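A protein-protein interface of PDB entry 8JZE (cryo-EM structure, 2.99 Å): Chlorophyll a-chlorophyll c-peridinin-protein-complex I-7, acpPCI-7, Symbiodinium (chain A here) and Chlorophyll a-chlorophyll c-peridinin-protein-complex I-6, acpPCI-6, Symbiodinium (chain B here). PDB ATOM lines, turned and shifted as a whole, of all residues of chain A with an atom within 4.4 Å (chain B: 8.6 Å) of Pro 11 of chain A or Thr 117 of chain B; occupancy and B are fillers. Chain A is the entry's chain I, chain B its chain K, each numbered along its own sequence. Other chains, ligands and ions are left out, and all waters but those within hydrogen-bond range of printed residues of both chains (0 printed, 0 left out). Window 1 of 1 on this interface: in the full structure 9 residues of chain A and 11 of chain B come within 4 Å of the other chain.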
ATOM      1  N   LYS A   1      -4.356  -4.347   9.988  1.00  0.00           N
ATOM      2  CA  LYS A   1      -4.737  -5.714   9.657  1.00  0.00           C
ATOM      3  C   LYS A   1      -6.202  -5.968   9.989  1.00  0.00           C
ATOM      4  O   LYS A   1      -6.552  -6.230  11.139  1.00  0.00           O
ATOM      5  CB  LYS A   1      -3.846  -6.713  10.395  1.00  0.00           C
ATOM      6  CG  LYS A   1      -2.381  -6.629  10.006  1.00  0.00           C
ATOM      7  CD  LYS A   1      -1.529  -7.567  10.841  1.00  0.00           C
ATOM      8  CE  LYS A   1      -1.597  -7.206  12.315  1.00  0.00           C
ATOM      9  NZ  LYS A   1      -0.693  -8.057  13.138  1.00  0.00           N
ATOM     10  N   GLU A   2      -7.052  -5.890   8.970  1.00  0.00           N
ATOM     11  CA  GLU A   2      -8.480  -6.081   9.166  1.00  0.00           C
ATOM     12  C   GLU A   2      -8.798  -7.547   9.446  1.00  0.00           C
ATOM     13  O   GLU A   2      -7.976  -8.444   9.238  1.00  0.00           O
ATOM     14  CB  GLU A   2      -9.257  -5.602   7.940  1.00  0.00           C
ATOM     15  N   THR A   3     -10.014  -7.780   9.929  1.00  0.00           N
ATOM     16  CA  THR A   3     -10.522  -9.118  10.181  1.00  0.00           C
ATOM     17  C   THR A   3     -11.776  -9.350   9.353  1.00  0.00           C
ATOM     18  O   THR A   3     -12.448  -8.408   8.925  1.00  0.00           O
ATOM     19  CB  THR A   3     -10.837  -9.334  11.667  1.00  0.00           C
ATOM     20  OG1 THR A   3     -11.898  -8.459  12.066  1.00  0.00           O
ATOM     21  CG2 THR A   3      -9.611  -9.056  12.518  1.00  0.00           C
ATOM     22  N   SER A   4     -12.083 -10.622   9.122  1.00  0.00           N
ATOM     23  CA  SER A   4     -13.283 -10.970   8.378  1.00  0.00           C
ATOM     24  C   SER A   4     -14.525 -10.612   9.183  1.00  0.00           C
ATOM     25  O   SER A   4     -14.541 -10.718  10.411  1.00  0.00           O
ATOM     26  CB  SER A   4     -13.291 -12.458   8.042  1.00  0.00           C
ATOM     27  OG  SER A   4     -13.256 -13.234   9.224  1.00  0.00           O
ATOM     28  N   LEU A  10     -10.383 -14.059  12.785  1.00  0.00           N
ATOM     29  CA  LEU A  10      -9.526 -14.487  11.696  1.00  0.00           C
ATOM     30  C   LEU A  10      -9.265 -13.325  10.745  1.00  0.00           C
ATOM     31  O   LEU A  10     -10.104 -12.428  10.612  1.00  0.00           O
ATOM     32  CB  LEU A  10     -10.157 -15.650  10.918  1.00  0.00           C
ATOM     33  CG  LEU A  10     -10.313 -16.968  11.677  1.00  0.00           C
ATOM     34  CD1 LEU A  10     -10.907 -18.041  10.784  1.00  0.00           C
ATOM     35  CD2 LEU A  10      -8.977 -17.418  12.229  1.00  0.00           C
ATOM     36  N   PRO A  11      -8.111 -13.308  10.080  1.00  0.00           N
ATOM     37  CA  PRO A  11      -7.822 -12.219   9.139  1.00  0.00           C
ATOM     38  C   PRO A  11      -8.807 -12.209   7.980  1.00  0.00           C
ATOM     39  O   PRO A  11      -9.317 -13.248   7.557  1.00  0.00           O
ATOM     40  CB  PRO A  11      -6.397 -12.527   8.664  1.00  0.00           C
ATOM     41  CG  PRO A  11      -6.212 -13.985   8.931  1.00  0.00           C
ATOM     42  CD  PRO A  11      -6.995 -14.262  10.176  1.00  0.00           C
ATOM     43  N   LYS A  12      -9.073 -11.011   7.473  1.00  0.00           N
ATOM     44  CA  LYS A  12     -10.012 -10.856   6.371  1.00  0.00           C
ATOM     45  C   LYS A  12      -9.472 -11.552   5.126  1.00  0.00           C
ATOM     46  O   LYS A  12      -8.345 -11.264   4.703  1.00  0.00           O
ATOM     47  CB  LYS A  12     -10.253  -9.375   6.085  1.00  0.00           C
ATOM     48  CG  LYS A  12     -11.043  -9.099   4.815  1.00  0.00           C
ATOM     49  CD  LYS A  12     -11.053  -7.612   4.492  1.00  0.00           C
ATOM     50  CE  LYS A  12     -11.847  -7.321   3.231  1.00  0.00           C
ATOM     51  NZ  LYS A  12     -13.274  -7.712   3.376  1.00  0.00           N
ATOM     52  N   PRO A  13     -10.232 -12.463   4.518  1.00  0.00           N
ATOM     53  CA  PRO A  13      -9.725 -13.166   3.332  1.00  0.00           C
ATOM     54  C   PRO A  13      -9.539 -12.249   2.137  1.00  0.00           C
ATOM     55  O   PRO A  13     -10.510 -11.709   1.599  1.00  0.00           O
ATOM     56  CB  PRO A  13     -10.808 -14.219   3.059  1.00  0.00           C
ATOM     57  CG  PRO A  13     -11.540 -14.367   4.343  1.00  0.00           C
ATOM     58  CD  PRO A  13     -11.521 -13.008   4.969  1.00  0.00           C
ATOM     59  N   ARG B  41       1.237 -15.608  25.630  1.00  0.00           N
ATOM     60  CA  ARG B  41       0.001 -15.626  24.854  1.00  0.00           C
ATOM     61  C   ARG B  41      -0.595 -17.027  24.790  1.00  0.00           C
ATOM     62  O   ARG B  41      -1.803 -17.203  24.993  1.00  0.00           O
ATOM     63  CB  ARG B  41       0.268 -15.080  23.450  1.00  0.00           C
ATOM     64  CG  ARG B  41      -0.593 -13.886  23.076  1.00  0.00           C
ATOM     65  CD  ARG B  41       0.127 -12.918  22.144  1.00  0.00           C
ATOM     66  NE  ARG B  41       0.601 -13.558  20.922  1.00  0.00           N
ATOM     67  CZ  ARG B  41       1.873 -13.821  20.660  1.00  0.00           C
ATOM     68  NH1 ARG B  41       2.834 -13.505  21.512  1.00  0.00           N
ATOM     69  NH2 ARG B  41       2.189 -14.417  19.515  1.00  0.00           N
ATOM     70  N   LEU B 108      -7.050 -22.177  13.949  1.00  0.00           N
ATOM     71  CA  LEU B 108      -6.779 -21.134  12.966  1.00  0.00           C
ATOM     72  C   LEU B 108      -6.581 -19.786  13.647  1.00  0.00           C
ATOM     73  O   LEU B 108      -5.689 -19.015  13.271  1.00  0.00           O
ATOM     74  CB  LEU B 108      -7.910 -21.066  11.941  1.00  0.00           C
ATOM     75  CG  LEU B 108      -8.024 -22.257  10.988  1.00  0.00           C
ATOM     76  CD1 LEU B 108      -9.161 -22.058  10.002  1.00  0.00           C
ATOM     77  CD2 LEU B 108      -6.716 -22.470  10.252  1.00  0.00           C
ATOM     78  N   ALA B 109      -7.401 -19.491  14.659  1.00  0.00           N
ATOM     79  CA  ALA B 109      -7.251 -18.242  15.400  1.00  0.00           C
ATOM     80  C   ALA B 109      -5.881 -18.158  16.059  1.00  0.00           C
ATOM     81  O   ALA B 109      -5.204 -17.126  15.987  1.00  0.00           O
ATOM     82  CB  ALA B 109      -8.360 -18.117  16.444  1.00  0.00           C
ATOM     83  N   ILE B 110      -5.449 -19.247  16.698  1.00  0.00           N
ATOM     84  CA  ILE B 110      -4.150 -19.256  17.364  1.00  0.00           C
ATOM     85  C   ILE B 110      -3.024 -19.095  16.355  1.00  0.00           C
ATOM     86  O   ILE B 110      -2.078 -18.332  16.577  1.00  0.00           O
ATOM     87  CB  ILE B 110      -3.975 -20.544  18.186  1.00  0.00           C
ATOM     88  CG1 ILE B 110      -4.873 -20.523  19.414  1.00  0.00           C
ATOM     89  CG2 ILE B 110      -2.524 -20.715  18.604  1.00  0.00           C
ATOM     90  CD1 ILE B 110      -4.531 -21.607  20.379  1.00  0.00           C
ATOM     91  N   THR B 111      -3.097 -19.821  15.238  1.00  0.00           N
ATOM     92  CA  THR B 111      -2.037 -19.743  14.239  1.00  0.00           C
ATOM     93  C   THR B 111      -1.937 -18.343  13.651  1.00  0.00           C
ATOM     94  O   THR B 111      -0.833 -17.813  13.473  1.00  0.00           O
ATOM     95  CB  THR B 111      -2.276 -20.777  13.139  1.00  0.00           C
ATOM     96  OG1 THR B 111      -2.231 -22.094  13.702  1.00  0.00           O
ATOM     97  CG2 THR B 111      -1.216 -20.665  12.058  1.00  0.00           C
ATOM     98  N   ASN B 112      -3.077 -17.717  13.356  1.00  0.00           N
ATOM     99  CA  ASN B 112      -3.064 -16.384  12.770  1.00  0.00           C
ATOM    100  C   ASN B 112      -2.776 -15.288  13.790  1.00  0.00           C
ATOM    101  O   ASN B 112      -2.415 -14.176  13.393  1.00  0.00           O
ATOM    102  CB  ASN B 112      -4.396 -16.108  12.068  1.00  0.00           C
ATOM    103  CG  ASN B 112      -4.598 -16.980  10.841  1.00  0.00           C
ATOM    104  OD1 ASN B 112      -5.555 -17.749  10.762  1.00  0.00           O
ATOM    105  ND2 ASN B 112      -3.695 -16.862   9.875  1.00  0.00           N
ATOM    106  N   MET B 113      -2.927 -15.568  15.085  1.00  0.00           N
ATOM    107  CA  MET B 113      -2.556 -14.597  16.108  1.00  0.00           C
ATOM    108  C   MET B 113      -1.079 -14.679  16.471  1.00  0.00           C
ATOM    109  O   MET B 113      -0.414 -13.647  16.602  1.00  0.00           O
ATOM    110  CB  MET B 113      -3.412 -14.799  17.361  1.00  0.00           C
ATOM    111  CG  MET B 113      -2.973 -13.974  18.560  1.00  0.00           C
ATOM    112  SD  MET B 113      -2.076 -14.926  19.800  1.00  0.00           S
ATOM    113  CE  MET B 113      -3.388 -15.943  20.469  1.00  0.00           C
ATOM    114  N   MET B 114      -0.553 -15.895  16.629  1.00  0.00           N
ATOM    115  CA  MET B 114       0.851 -16.065  16.982  1.00  0.00           C
ATOM    116  C   MET B 114       1.769 -15.600  15.859  1.00  0.00           C
ATOM    117  O   MET B 114       2.864 -15.092  16.125  1.00  0.00           O
ATOM    118  CB  MET B 114       1.123 -17.528  17.330  1.00  0.00           C
ATOM    119  CG  MET B 114       2.195 -17.734  18.383  1.00  0.00           C
ATOM    120  SD  MET B 114       1.649 -17.287  20.039  1.00  0.00           S
ATOM    121  CE  MET B 114       0.391 -18.527  20.319  1.00  0.00           C
ATOM    122  N   GLU B 115       1.345 -15.765  14.606  1.00  0.00           N
ATOM    123  CA  GLU B 115       2.108 -15.270  13.470  1.00  0.00           C
ATOM    124  C   GLU B 115       1.898 -13.784  13.220  1.00  0.00           C
ATOM    125  O   GLU B 115       2.574 -13.217  12.357  1.00  0.00           O
ATOM    126  CB  GLU B 115       1.748 -16.049  12.202  1.00  0.00           C
ATOM    127  CG  GLU B 115       2.254 -17.478  12.177  1.00  0.00           C
ATOM    128  CD  GLU B 115       2.009 -18.155  10.843  1.00  0.00           C
ATOM    129  OE1 GLU B 115       1.206 -17.630  10.043  1.00  0.00           O
ATOM    130  OE2 GLU B 115       2.625 -19.210  10.592  1.00  0.00           O
ATOM    131  N   GLY B 116       0.980 -13.147  13.942  1.00  0.00           N
ATOM    132  CA  GLY B 116       0.749 -11.730  13.773  1.00  0.00           C
ATOM    133  C   GLY B 116      -0.093 -11.353  12.578  1.00  0.00           C
ATOM    134  O   GLY B 116      -0.237 -10.159  12.299  1.00  0.00           O
ATOM    135  N   THR B 117      -0.651 -12.330  11.857  1.00  0.00           N
ATOM    136  CA  THR B 117      -1.506 -12.010  10.718  1.00  0.00           C
ATOM    137  C   THR B 117      -2.734 -11.220  11.151  1.00  0.00           C
ATOM    138  O   THR B 117      -3.211 -10.356  10.406  1.00  0.00           O
ATOM    139  CB  THR B 117      -1.916 -13.295   9.995  1.00  0.00           C
ATOM    140  OG1 THR B 117      -0.743 -14.040   9.643  1.00  0.00           O
ATOM    141  CG2 THR B 117      -2.685 -12.974   8.729  1.00  0.00           C
ATOM    142  N   THR B 118      -3.246 -11.487  12.345  1.00  0.00           N
ATOM    143  CA  THR B 118      -4.312 -10.707  12.956  1.00  0.00           C
ATOM    144  C   THR B 118      -3.779 -10.050  14.228  1.00  0.00           C
ATOM    145  O   THR B 118      -2.633 -10.262  14.629  1.00  0.00           O
ATOM    146  CB  THR B 118      -5.533 -11.583  13.255  1.00  0.00           C
ATOM    147  OG1 THR B 118      -6.624 -10.757  13.681  1.00  0.00           O
ATOM    148  CG2 THR B 118      -5.214 -12.588  14.347  1.00  0.00           C
ATOM    149  N   ASP B 119      -4.625  -9.242  14.861  1.00  0.00           N
ATOM    150  CA  ASP B 119      -4.283  -8.520  16.081  1.00  0.00           C
ATOM    151  C   ASP B 119      -5.129  -9.017  17.247  1.00  0.00           C
ATOM    152  O   ASP B 119      -5.659  -8.235  18.040  1.00  0.00           O
ATOM    153  CB  ASP B 119      -4.449  -7.014  15.888  1.00  0.00           C
ATOM    154  CG  ASP B 119      -3.762  -6.204  16.973  1.00  0.00           C
ATOM    155  OD1 ASP B 119      -3.018  -6.797  17.783  1.00  0.00           O
ATOM    156  OD2 ASP B 119      -3.971  -4.973  17.019  1.00  0.00           O
ATOM    157  N   ARG B 120      -5.263 -10.335  17.359  1.00  0.00           N
ATOM    158  CA  ARG B 120      -6.176 -10.940  18.318  1.00  0.00           C
ATOM    159  C   ARG B 120      -5.537 -11.020  19.699  1.00  0.00           C
ATOM    160  O   ARG B 120      -4.375 -11.416  19.834  1.00  0.00           O
ATOM    161  CB  ARG B 120      -6.580 -12.335  17.845  1.00  0.00           C
ATOM    162  CG  ARG B 120      -7.787 -12.926  18.553  1.00  0.00           C
ATOM    163  CD  ARG B 120      -8.042 -14.354  18.092  1.00  0.00           C
ATOM    164  NE  ARG B 120      -7.209 -15.317  18.799  1.00  0.00           N
ATOM    165  CZ  ARG B 120      -7.624 -16.068  19.811  1.00  0.00           C
ATOM    166  NH1 ARG B 120      -8.869 -16.004  20.251  1.00  0.00           N
ATOM    167  NH2 ARG B 120      -6.769 -16.901  20.396  1.00  0.00           N
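Pro 11 of chain A touches just these residues of chain B: Asn 112 and Thr 117. Thr 117 of chain B touches just these residues of chain A: Lys 1 and Pro 11. Of the printed residues of chain A, Gly 116 of chain B touches Lys 1. Of the printed residues of chain A, Asn 112 of chain B touches Leu 10 (3.7 Å) and Pro 11 (3.7 Å). Of the printed residues of chain A, Thr 118 of chain B touches Lys 1 and Thr 3. Printed residues of chain B within 4 Å of Thr 3 of chain A: Thr 118 (3.6 Å). Glu 2 of chain A touches none of the printed residues of chain B. The nearest printed residue of chain A that does not touch Thr 117 of chain B is Glu 2 of chain A (5.3 Å).
The backbone carbonyl oxygen (O) of Thr 118 of chain B sits at hydrogen-bond distance from the side-chain amino group (NZ) of Lys 1 of chain A (3.3 Å). NZ of Lys 1 of chain A sits close to O of Gly 116 of chain B, 2.3 Å away.
Printed residues of chain A that touch a printed residue of chain B: Lys 1, Thr 3, Leu 10 and Pro 11. Hydrophobic or aromatic side chains of chain A that line the printed part of chain B: Leu 10 and Pro 11. Along chain B the printed residues that touch a printed residue of chain A span positions 108 to 118. Among the printed residues, 9 pairs touch across the chains.
Lys 1 of chain A touches Thr 117 of chain B. Thr 3 of chain A touches Thr 118 of chain B (CG2 to OG1, 3.6 Å). Leu 10 of chain A touches Leu 108 of chain B. N of Ala 109 of chain B touches CD2 of Leu 10 of chain A, at 3.6 Å. Asn 112 of chain B touches Leu 10 of chain A (OD1 to CD2, 3.7 Å). Asn 112 of chain B touches Pro 11 of chain A. Thr 117 of chain B touches Pro 11 of chain A (CG2 to CG, 3.7 Å).
The backbone carbonyl oxygen (O) of Leu 108 of chain B sits close to the side-chain amide oxygen (OD1) of Asn 112 of chain B (2.8 Å). The backbone carbonyl oxygen (O) of Leu 10 of chain A sits at hydrogen-bond distance from the backbone NH (N) of Ser 4 of chain A. N of Thr 117 of chain B lies within hydrogen-bond range of O of Asn 112 of chain B, 3.0 Å away. The backbone carbonyl oxygen of Asn 112 of chain B lies within hydrogen-bond range of the backbone NH of Thr 118 of chain B (3.0 Å).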
